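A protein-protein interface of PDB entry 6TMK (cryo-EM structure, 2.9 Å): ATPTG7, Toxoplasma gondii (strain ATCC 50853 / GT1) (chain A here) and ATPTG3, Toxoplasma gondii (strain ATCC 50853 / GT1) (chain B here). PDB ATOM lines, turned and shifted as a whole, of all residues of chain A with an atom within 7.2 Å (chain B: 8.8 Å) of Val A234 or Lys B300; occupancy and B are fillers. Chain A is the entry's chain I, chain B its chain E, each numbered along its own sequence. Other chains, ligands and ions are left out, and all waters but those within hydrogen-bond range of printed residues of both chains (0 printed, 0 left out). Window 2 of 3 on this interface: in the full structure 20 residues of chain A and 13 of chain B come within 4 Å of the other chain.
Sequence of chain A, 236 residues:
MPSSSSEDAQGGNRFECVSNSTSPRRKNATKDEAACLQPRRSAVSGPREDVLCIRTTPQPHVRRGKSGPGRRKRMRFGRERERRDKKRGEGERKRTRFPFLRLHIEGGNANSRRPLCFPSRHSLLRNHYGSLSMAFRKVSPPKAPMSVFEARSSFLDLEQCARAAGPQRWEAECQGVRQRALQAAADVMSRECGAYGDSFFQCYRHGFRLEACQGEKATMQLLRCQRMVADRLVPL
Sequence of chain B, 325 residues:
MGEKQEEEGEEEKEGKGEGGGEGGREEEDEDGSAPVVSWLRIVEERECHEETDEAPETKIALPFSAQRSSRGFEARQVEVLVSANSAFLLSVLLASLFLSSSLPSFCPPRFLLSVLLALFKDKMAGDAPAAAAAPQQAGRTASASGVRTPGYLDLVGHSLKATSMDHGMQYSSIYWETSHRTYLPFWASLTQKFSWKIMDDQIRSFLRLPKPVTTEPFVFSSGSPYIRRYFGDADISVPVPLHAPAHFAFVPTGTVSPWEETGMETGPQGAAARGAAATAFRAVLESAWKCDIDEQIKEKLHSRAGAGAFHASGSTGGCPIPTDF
The side-chain amino group of Lys B300 is in hydrogen-bond range of the backbone carbonyl oxygen of Val A234 (3.2 Å).
OG of Ser B303 is in hydrogen-bond range of O of Lys B300, at 2.7 Å.
CE1 of Phe A155 touches CD1 of Ile B297, at 3.9 Å. O of Ala A185 touches CZ3 of Trp B289, at 3.3 Å. CZ2 of Trp B289 touches CG1 of Val A229 (3.9 Å). CD1 of Ile B293 touches CB of Ala A230, 3.8 Å away. CG2 of Val A234 touches CD1 of Ile B297 (3.5 Å).
Val A234 touches just these residues of chain B: Ile B297 and Lys B300. Of chain A, only Val A234 (3.2 Å) comes within 4 Å of Lys B300. No residue of chain B comes within 4 Å of Pro A235. Printed residues of chain B within 4 Å of Val A229: Trp B289. Of the printed residues of chain A, Ile B293 touches Ala A230 (3.8 Å). Lys B298 touches none of the printed residues of chain A. The nearest residue of chain A that does not touch Lys B300 is Pro A235 (4.4 Å).
Printed residues of chain B that touch a printed residue of chain A: Trp B289, Ile B293, Ile B297 and Lys B300. Hydrophobic or aromatic side chains of chain B within 4 Å of the printed part of chain A: Trp B289, Ile B293 and Ile B297. Of the 12 printed residues of chain A, 5 touch a printed residue of chain B. Printed residues of chain A that touch a printed residue of chain B: Phe A155, Ala A185, Val A229, Ala A230 and Val A234. Hydrophobic or aromatic side chains of chain A within 4 Å of the printed part of chain B: Phe A155, Ala A185, Val A229, Ala A230 and Val A234. Among the printed residues, 6 pairs touch across the chains.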
ATOM      1  N   ARG A 152      24.120   0.711 -13.952  1.00  0.00           N
ATOM      2  CA  ARG A 152      25.492   0.676 -14.436  1.00  0.00           C
ATOM      3  C   ARG A 152      26.409   1.520 -13.557  1.00  0.00           C
ATOM      4  O   ARG A 152      27.523   1.097 -13.215  1.00  0.00           O
ATOM      5  CB  ARG A 152      25.507   1.149 -15.885  1.00  0.00           C
ATOM      6  CG  ARG A 152      26.804   0.959 -16.616  1.00  0.00           C
ATOM      7  CD  ARG A 152      26.601   1.351 -18.062  1.00  0.00           C
ATOM      8  NE  ARG A 152      25.714   0.406 -18.733  1.00  0.00           N
ATOM      9  CZ  ARG A 152      25.190   0.601 -19.937  1.00  0.00           C
ATOM     10  NH1 ARG A 152      25.456   1.711 -20.608  1.00  0.00           N
ATOM     11  NH2 ARG A 152      24.393  -0.314 -20.468  1.00  0.00           N
ATOM     12  N   PHE A 155      27.085  -0.417 -10.389  1.00  0.00           N
ATOM     13  CA  PHE A 155      28.101  -1.452 -10.539  1.00  0.00           C
ATOM     14  C   PHE A 155      29.496  -0.857 -10.679  1.00  0.00           C
ATOM     15  O   PHE A 155      30.474  -1.465 -10.230  1.00  0.00           O
ATOM     16  CB  PHE A 155      27.787  -2.331 -11.745  1.00  0.00           C
ATOM     17  CG  PHE A 155      26.768  -3.390 -11.471  1.00  0.00           C
ATOM     18  CD1 PHE A 155      27.123  -4.552 -10.815  1.00  0.00           C
ATOM     19  CD2 PHE A 155      25.457  -3.230 -11.873  1.00  0.00           C
ATOM     20  CE1 PHE A 155      26.190  -5.531 -10.562  1.00  0.00           C
ATOM     21  CE2 PHE A 155      24.521  -4.207 -11.622  1.00  0.00           C
ATOM     22  CZ  PHE A 155      24.889  -5.359 -10.967  1.00  0.00           C
ATOM     23  N   LEU A 156      29.612   0.334 -11.264  1.00  0.00           N
ATOM     24  CA  LEU A 156      30.923   0.974 -11.332  1.00  0.00           C
ATOM     25  C   LEU A 156      31.394   1.422  -9.953  1.00  0.00           C
ATOM     26  O   LEU A 156      32.569   1.245  -9.601  1.00  0.00           O
ATOM     27  CB  LEU A 156      30.883   2.159 -12.291  1.00  0.00           C
ATOM     28  CG  LEU A 156      31.390   1.849 -13.698  1.00  0.00           C
ATOM     29  CD1 LEU A 156      30.408   0.975 -14.451  1.00  0.00           C
ATOM     30  CD2 LEU A 156      31.651   3.141 -14.446  1.00  0.00           C
ATOM     31  N   GLU A 159      32.625  -1.740  -8.282  1.00  0.00           N
ATOM     32  CA  GLU A 159      33.912  -2.259  -8.724  1.00  0.00           C
ATOM     33  C   GLU A 159      35.053  -1.366  -8.256  1.00  0.00           C
ATOM     34  O   GLU A 159      36.108  -1.863  -7.846  1.00  0.00           O
ATOM     35  CB  GLU A 159      33.930  -2.413 -10.243  1.00  0.00           C
ATOM     36  CG  GLU A 159      34.385  -1.180 -11.003  1.00  0.00           C
ATOM     37  CD  GLU A 159      34.192  -1.314 -12.499  1.00  0.00           C
ATOM     38  OE1 GLU A 159      33.321  -2.105 -12.920  1.00  0.00           O
ATOM     39  OE2 GLU A 159      34.914  -0.630 -13.255  1.00  0.00           O
ATOM     40  N   ALA A 185      19.737  -3.752 -10.648  1.00  0.00           N
ATOM     41  CA  ALA A 185      19.738  -4.762 -11.700  1.00  0.00           C
ATOM     42  C   ALA A 185      18.460  -5.588 -11.670  1.00  0.00           C
ATOM     43  O   ALA A 185      17.936  -5.977 -12.718  1.00  0.00           O
ATOM     44  CB  ALA A 185      20.961  -5.659 -11.555  1.00  0.00           C
ATOM     45  N   VAL A 229      20.133  -9.235 -20.029  1.00  0.00           N
ATOM     46  CA  VAL A 229      20.176  -8.157 -19.047  1.00  0.00           C
ATOM     47  C   VAL A 229      21.484  -8.200 -18.268  1.00  0.00           C
ATOM     48  O   VAL A 229      22.140  -7.171 -18.061  1.00  0.00           O
ATOM     49  CB  VAL A 229      18.962  -8.242 -18.108  1.00  0.00           C
ATOM     50  CG1 VAL A 229      19.160  -7.341 -16.915  1.00  0.00           C
ATOM     51  CG2 VAL A 229      17.707  -7.864 -18.851  1.00  0.00           C
ATOM     52  N   ALA A 230      21.882  -9.389 -17.821  1.00  0.00           N
ATOM     53  CA  ALA A 230      23.130  -9.507 -17.078  1.00  0.00           C
ATOM     54  C   ALA A 230      24.318  -9.078 -17.931  1.00  0.00           C
ATOM     55  O   ALA A 230      25.150  -8.268 -17.503  1.00  0.00           O
ATOM     56  CB  ALA A 230      23.308 -10.941 -16.586  1.00  0.00           C
ATOM     57  N   ASP A 231      24.407  -9.607 -19.153  1.00  0.00           N
ATOM     58  CA  ASP A 231      25.506  -9.257 -20.046  1.00  0.00           C
ATOM     59  C   ASP A 231      25.536  -7.767 -20.349  1.00  0.00           C
ATOM     60  O   ASP A 231      26.606  -7.207 -20.611  1.00  0.00           O
ATOM     61  CB  ASP A 231      25.392 -10.054 -21.341  1.00  0.00           C
ATOM     62  CG  ASP A 231      25.595 -11.539 -21.130  1.00  0.00           C
ATOM     63  OD1 ASP A 231      25.960 -11.936 -20.004  1.00  0.00           O
ATOM     64  OD2 ASP A 231      25.393 -12.312 -22.090  1.00  0.00           O
ATOM     65  N   ARG A 232      24.381  -7.109 -20.327  1.00  0.00           N
ATOM     66  CA  ARG A 232      24.330  -5.672 -20.552  1.00  0.00           C
ATOM     67  C   ARG A 232      24.750  -4.884 -19.321  1.00  0.00           C
ATOM     68  O   ARG A 232      25.301  -3.787 -19.452  1.00  0.00           O
ATOM     69  CB  ARG A 232      22.921  -5.260 -20.970  1.00  0.00           C
ATOM     70  CG  ARG A 232      22.867  -4.020 -21.827  1.00  0.00           C
ATOM     71  CD  ARG A 232      21.435  -3.635 -22.133  1.00  0.00           C
ATOM     72  NE  ARG A 232      20.739  -4.686 -22.872  1.00  0.00           N
ATOM     73  CZ  ARG A 232      19.528  -5.153 -22.575  1.00  0.00           C
ATOM     74  NH1 ARG A 232      18.839  -4.662 -21.554  1.00  0.00           N
ATOM     75  NH2 ARG A 232      18.995  -6.111 -23.317  1.00  0.00           N
ATOM     76  N   LEU A 233      24.495  -5.416 -18.128  1.00  0.00           N
ATOM     77  CA  LEU A 233      24.740  -4.669 -16.901  1.00  0.00           C
ATOM     78  C   LEU A 233      26.143  -4.885 -16.339  1.00  0.00           C
ATOM     79  O   LEU A 233      26.918  -3.932 -16.216  1.00  0.00           O
ATOM     80  CB  LEU A 233      23.703  -5.052 -15.843  1.00  0.00           C
ATOM     81  CG  LEU A 233      22.264  -4.643 -16.133  1.00  0.00           C
ATOM     82  CD1 LEU A 233      21.349  -5.226 -15.084  1.00  0.00           C
ATOM     83  CD2 LEU A 233      22.138  -3.143 -16.173  1.00  0.00           C
ATOM     84  N   VAL A 234      26.484  -6.121 -15.992  1.00  0.00           N
ATOM     85  CA  VAL A 234      27.634  -6.353 -15.118  1.00  0.00           C
ATOM     86  C   VAL A 234      28.959  -6.102 -15.834  1.00  0.00           C
ATOM     87  O   VAL A 234      29.882  -5.556 -15.213  1.00  0.00           O
ATOM     88  CB  VAL A 234      27.602  -7.766 -14.511  1.00  0.00           C
ATOM     89  CG1 VAL A 234      27.744  -8.841 -15.573  1.00  0.00           C
ATOM     90  CG2 VAL A 234      28.690  -7.908 -13.468  1.00  0.00           C
ATOM     91  N   PRO A 235      29.127  -6.468 -17.115  1.00  0.00           N
ATOM     92  CA  PRO A 235      30.475  -6.242 -17.648  1.00  0.00           C
ATOM     93  C   PRO A 235      30.762  -4.769 -17.924  1.00  0.00           C
ATOM     94  O   PRO A 235      31.229  -4.071 -17.021  1.00  0.00           O
ATOM     95  CB  PRO A 235      30.483  -7.055 -18.954  1.00  0.00           C
ATOM     96  CG  PRO A 235      29.162  -7.797 -18.988  1.00  0.00           C
ATOM     97  CD  PRO A 235      28.232  -6.982 -18.158  1.00  0.00           C
ATOM     98  N   TRP B 289      17.499 -14.705  -9.364  1.00  0.00           N
ATOM     99  CA  TRP B 289      18.418 -14.000 -10.245  1.00  0.00           C
ATOM    100  C   TRP B 289      19.486 -13.267  -9.450  1.00  0.00           C
ATOM    101  O   TRP B 289      20.657 -13.239  -9.846  1.00  0.00           O
ATOM    102  CB  TRP B 289      17.627 -13.033 -11.119  1.00  0.00           C
ATOM    103  CG  TRP B 289      18.387 -12.477 -12.260  1.00  0.00           C
ATOM    104  CD1 TRP B 289      18.742 -13.127 -13.396  1.00  0.00           C
ATOM    105  CD2 TRP B 289      18.881 -11.144 -12.387  1.00  0.00           C
ATOM    106  NE1 TRP B 289      19.432 -12.285 -14.227  1.00  0.00           N
ATOM    107  CE2 TRP B 289      19.530 -11.058 -13.628  1.00  0.00           C
ATOM    108  CE3 TRP B 289      18.837 -10.014 -11.572  1.00  0.00           C
ATOM    109  CZ2 TRP B 289      20.132  -9.892 -14.071  1.00  0.00           C
ATOM    110  CZ3 TRP B 289      19.437  -8.859 -12.014  1.00  0.00           C
ATOM    111  CH2 TRP B 289      20.074  -8.805 -13.251  1.00  0.00           C
ATOM    112  N   ILE B 293      23.523 -13.740  -9.801  1.00  0.00           N
ATOM    113  CA  ILE B 293      24.392 -12.621 -10.142  1.00  0.00           C
ATOM    114  C   ILE B 293      25.375 -12.324  -9.023  1.00  0.00           C
ATOM    115  O   ILE B 293      26.494 -11.869  -9.282  1.00  0.00           O
ATOM    116  CB  ILE B 293      23.542 -11.385 -10.473  1.00  0.00           C
ATOM    117  CG1 ILE B 293      22.686 -11.645 -11.708  1.00  0.00           C
ATOM    118  CG2 ILE B 293      24.424 -10.183 -10.689  1.00  0.00           C
ATOM    119  CD1 ILE B 293      23.464 -11.927 -12.956  1.00  0.00           C
ATOM    120  N   ASP B 294      25.004 -12.589  -7.772  1.00  0.00           N
ATOM    121  CA  ASP B 294      25.956 -12.441  -6.681  1.00  0.00           C
ATOM    122  C   ASP B 294      27.088 -13.449  -6.813  1.00  0.00           C
ATOM    123  O   ASP B 294      28.258 -13.111  -6.603  1.00  0.00           O
ATOM    124  CB  ASP B 294      25.245 -12.597  -5.342  1.00  0.00           C
ATOM    125  CG  ASP B 294      26.117 -12.201  -4.170  1.00  0.00           C
ATOM    126  OD1 ASP B 294      27.277 -11.798  -4.401  1.00  0.00           O
ATOM    127  OD2 ASP B 294      25.643 -12.289  -3.019  1.00  0.00           O
ATOM    128  N   GLU B 295      26.756 -14.690  -7.168  1.00  0.00           N
ATOM    129  CA  GLU B 295      27.800 -15.682  -7.417  1.00  0.00           C
ATOM    130  C   GLU B 295      28.733 -15.232  -8.536  1.00  0.00           C
ATOM    131  O   GLU B 295      29.963 -15.343  -8.426  1.00  0.00           O
ATOM    132  CB  GLU B 295      27.170 -17.027  -7.763  1.00  0.00           C
ATOM    133  CG  GLU B 295      26.785 -17.852  -6.555  1.00  0.00           C
ATOM    134  CD  GLU B 295      26.260 -19.221  -6.932  1.00  0.00           C
ATOM    135  OE1 GLU B 295      26.007 -19.452  -8.134  1.00  0.00           O
ATOM    136  OE2 GLU B 295      26.101 -20.068  -6.028  1.00  0.00           O
ATOM    137  N   GLN B 296      28.160 -14.742  -9.637  1.00  0.00           N
ATOM    138  CA  GLN B 296      28.989 -14.293 -10.752  1.00  0.00           C
ATOM    139  C   GLN B 296      29.882 -13.126 -10.352  1.00  0.00           C
ATOM    140  O   GLN B 296      31.061 -13.081 -10.723  1.00  0.00           O
ATOM    141  CB  GLN B 296      28.108 -13.901 -11.935  1.00  0.00           C
ATOM    142  CG  GLN B 296      27.462 -15.077 -12.633  1.00  0.00           C
ATOM    143  CD  GLN B 296      26.579 -14.651 -13.785  1.00  0.00           C
ATOM    144  OE1 GLN B 296      26.952 -13.791 -14.582  1.00  0.00           O
ATOM    145  NE2 GLN B 296      25.400 -15.251 -13.876  1.00  0.00           N
ATOM    146  N   ILE B 297      29.344 -12.171  -9.593  1.00  0.00           N
ATOM    147  CA  ILE B 297      30.155 -11.061  -9.104  1.00  0.00           C
ATOM    148  C   ILE B 297      31.302 -11.574  -8.248  1.00  0.00           C
ATOM    149  O   ILE B 297      32.444 -11.109  -8.364  1.00  0.00           O
ATOM    150  CB  ILE B 297      29.275 -10.068  -8.328  1.00  0.00           C
ATOM    151  CG1 ILE B 297      28.363  -9.314  -9.293  1.00  0.00           C
ATOM    152  CG2 ILE B 297      30.138  -9.114  -7.529  1.00  0.00           C
ATOM    153  CD1 ILE B 297      29.032  -8.169 -10.001  1.00  0.00           C
ATOM    154  N   LYS B 298      31.016 -12.531  -7.366  1.00  0.00           N
ATOM    155  CA  LYS B 298      32.050 -13.055  -6.482  1.00  0.00           C
ATOM    156  C   LYS B 298      33.180 -13.678  -7.283  1.00  0.00           C
ATOM    157  O   LYS B 298      34.360 -13.378  -7.058  1.00  0.00           O
ATOM    158  CB  LYS B 298      31.461 -14.078  -5.516  1.00  0.00           C
ATOM    159  CG  LYS B 298      30.784 -13.470  -4.310  1.00  0.00           C
ATOM    160  CD  LYS B 298      30.580 -14.501  -3.215  1.00  0.00           C
ATOM    161  CE  LYS B 298      29.445 -15.451  -3.542  1.00  0.00           C
ATOM    162  NZ  LYS B 298      28.117 -14.784  -3.469  1.00  0.00           N
ATOM    163  N   GLU B 299      32.839 -14.547  -8.235  1.00  0.00           N
ATOM    164  CA  GLU B 299      33.893 -15.207  -8.997  1.00  0.00           C
ATOM    165  C   GLU B 299      34.624 -14.225  -9.901  1.00  0.00           C
ATOM    166  O   GLU B 299      35.820 -14.401 -10.161  1.00  0.00           O
ATOM    167  CB  GLU B 299      33.321 -16.368  -9.814  1.00  0.00           C
ATOM    168  CG  GLU B 299      32.273 -15.983 -10.843  1.00  0.00           C
ATOM    169  CD  GLU B 299      32.870 -15.462 -12.137  1.00  0.00           C
ATOM    170  OE1 GLU B 299      32.109 -14.923 -12.967  1.00  0.00           O
ATOM    171  OE2 GLU B 299      34.097 -15.596 -12.331  1.00  0.00           O
ATOM    172  N   LYS B 300      33.941 -13.186 -10.387  1.00  0.00           N
ATOM    173  CA  LYS B 300      34.615 -12.204 -11.228  1.00  0.00           C
ATOM    174  C   LYS B 300      35.616 -11.386 -10.422  1.00  0.00           C
ATOM    175  O   LYS B 300      36.725 -11.113 -10.895  1.00  0.00           O
ATOM    176  CB  LYS B 300      33.597 -11.283 -11.896  1.00  0.00           C
ATOM    177  CG  LYS B 300      34.230 -10.215 -12.771  1.00  0.00           C
ATOM    178  CD  LYS B 300      33.191  -9.443 -13.567  1.00  0.00           C
ATOM    179  CE  LYS B 300      32.721  -8.200 -12.829  1.00  0.00           C
ATOM    180  NZ  LYS B 300      32.224  -7.152 -13.764  1.00  0.00           N
ATOM    181  N   LEU B 301      35.244 -10.985  -9.207  1.00  0.00           N
ATOM    182  CA  LEU B 301      36.075 -10.080  -8.425  1.00  0.00           C
ATOM    183  C   LEU B 301      37.122 -10.796  -7.587  1.00  0.00           C
ATOM    184  O   LEU B 301      38.075 -10.152  -7.134  1.00  0.00           O
ATOM    185  CB  LEU B 301      35.207  -9.224  -7.503  1.00  0.00           C
ATOM    186  CG  LEU B 301      34.198  -8.311  -8.197  1.00  0.00           C
ATOM    187  CD1 LEU B 301      33.339  -7.601  -7.171  1.00  0.00           C
ATOM    188  CD2 LEU B 301      34.899  -7.312  -9.089  1.00  0.00           C
ATOM    189  N   HIS B 302      36.977 -12.104  -7.364  1.00  0.00           N
ATOM    190  CA  HIS B 302      38.073 -12.853  -6.759  1.00  0.00           C
ATOM    191  C   HIS B 302      39.262 -12.960  -7.703  1.00  0.00           C
ATOM    192  O   HIS B 302      40.413 -12.943  -7.253  1.00  0.00           O
ATOM    193  CB  HIS B 302      37.599 -14.243  -6.341  1.00  0.00           C
ATOM    194  CG  HIS B 302      37.067 -14.299  -4.944  1.00  0.00           C
ATOM    195  ND1 HIS B 302      37.767 -14.870  -3.903  1.00  0.00           N
ATOM    196  CD2 HIS B 302      35.907 -13.846  -4.412  1.00  0.00           C
ATOM    197  CE1 HIS B 302      37.060 -14.771  -2.792  1.00  0.00           C
ATOM    198  NE2 HIS B 302      35.926 -14.154  -3.073  1.00  0.00           N
ATOM    199  N   SER B 303      39.010 -13.070  -9.003  1.00  0.00           N
ATOM    200  CA  SER B 303      40.079 -13.053  -9.992  1.00  0.00           C
ATOM    201  C   SER B 303      40.799 -11.708  -9.978  1.00  0.00           C
ATOM    202  O   SER B 303      40.239 -10.698  -9.549  1.00  0.00           O
ATOM    203  CB  SER B 303      39.521 -13.334 -11.387  1.00  0.00           C
ATOM    204  OG  SER B 303      39.015 -12.152 -11.978  1.00  0.00           O
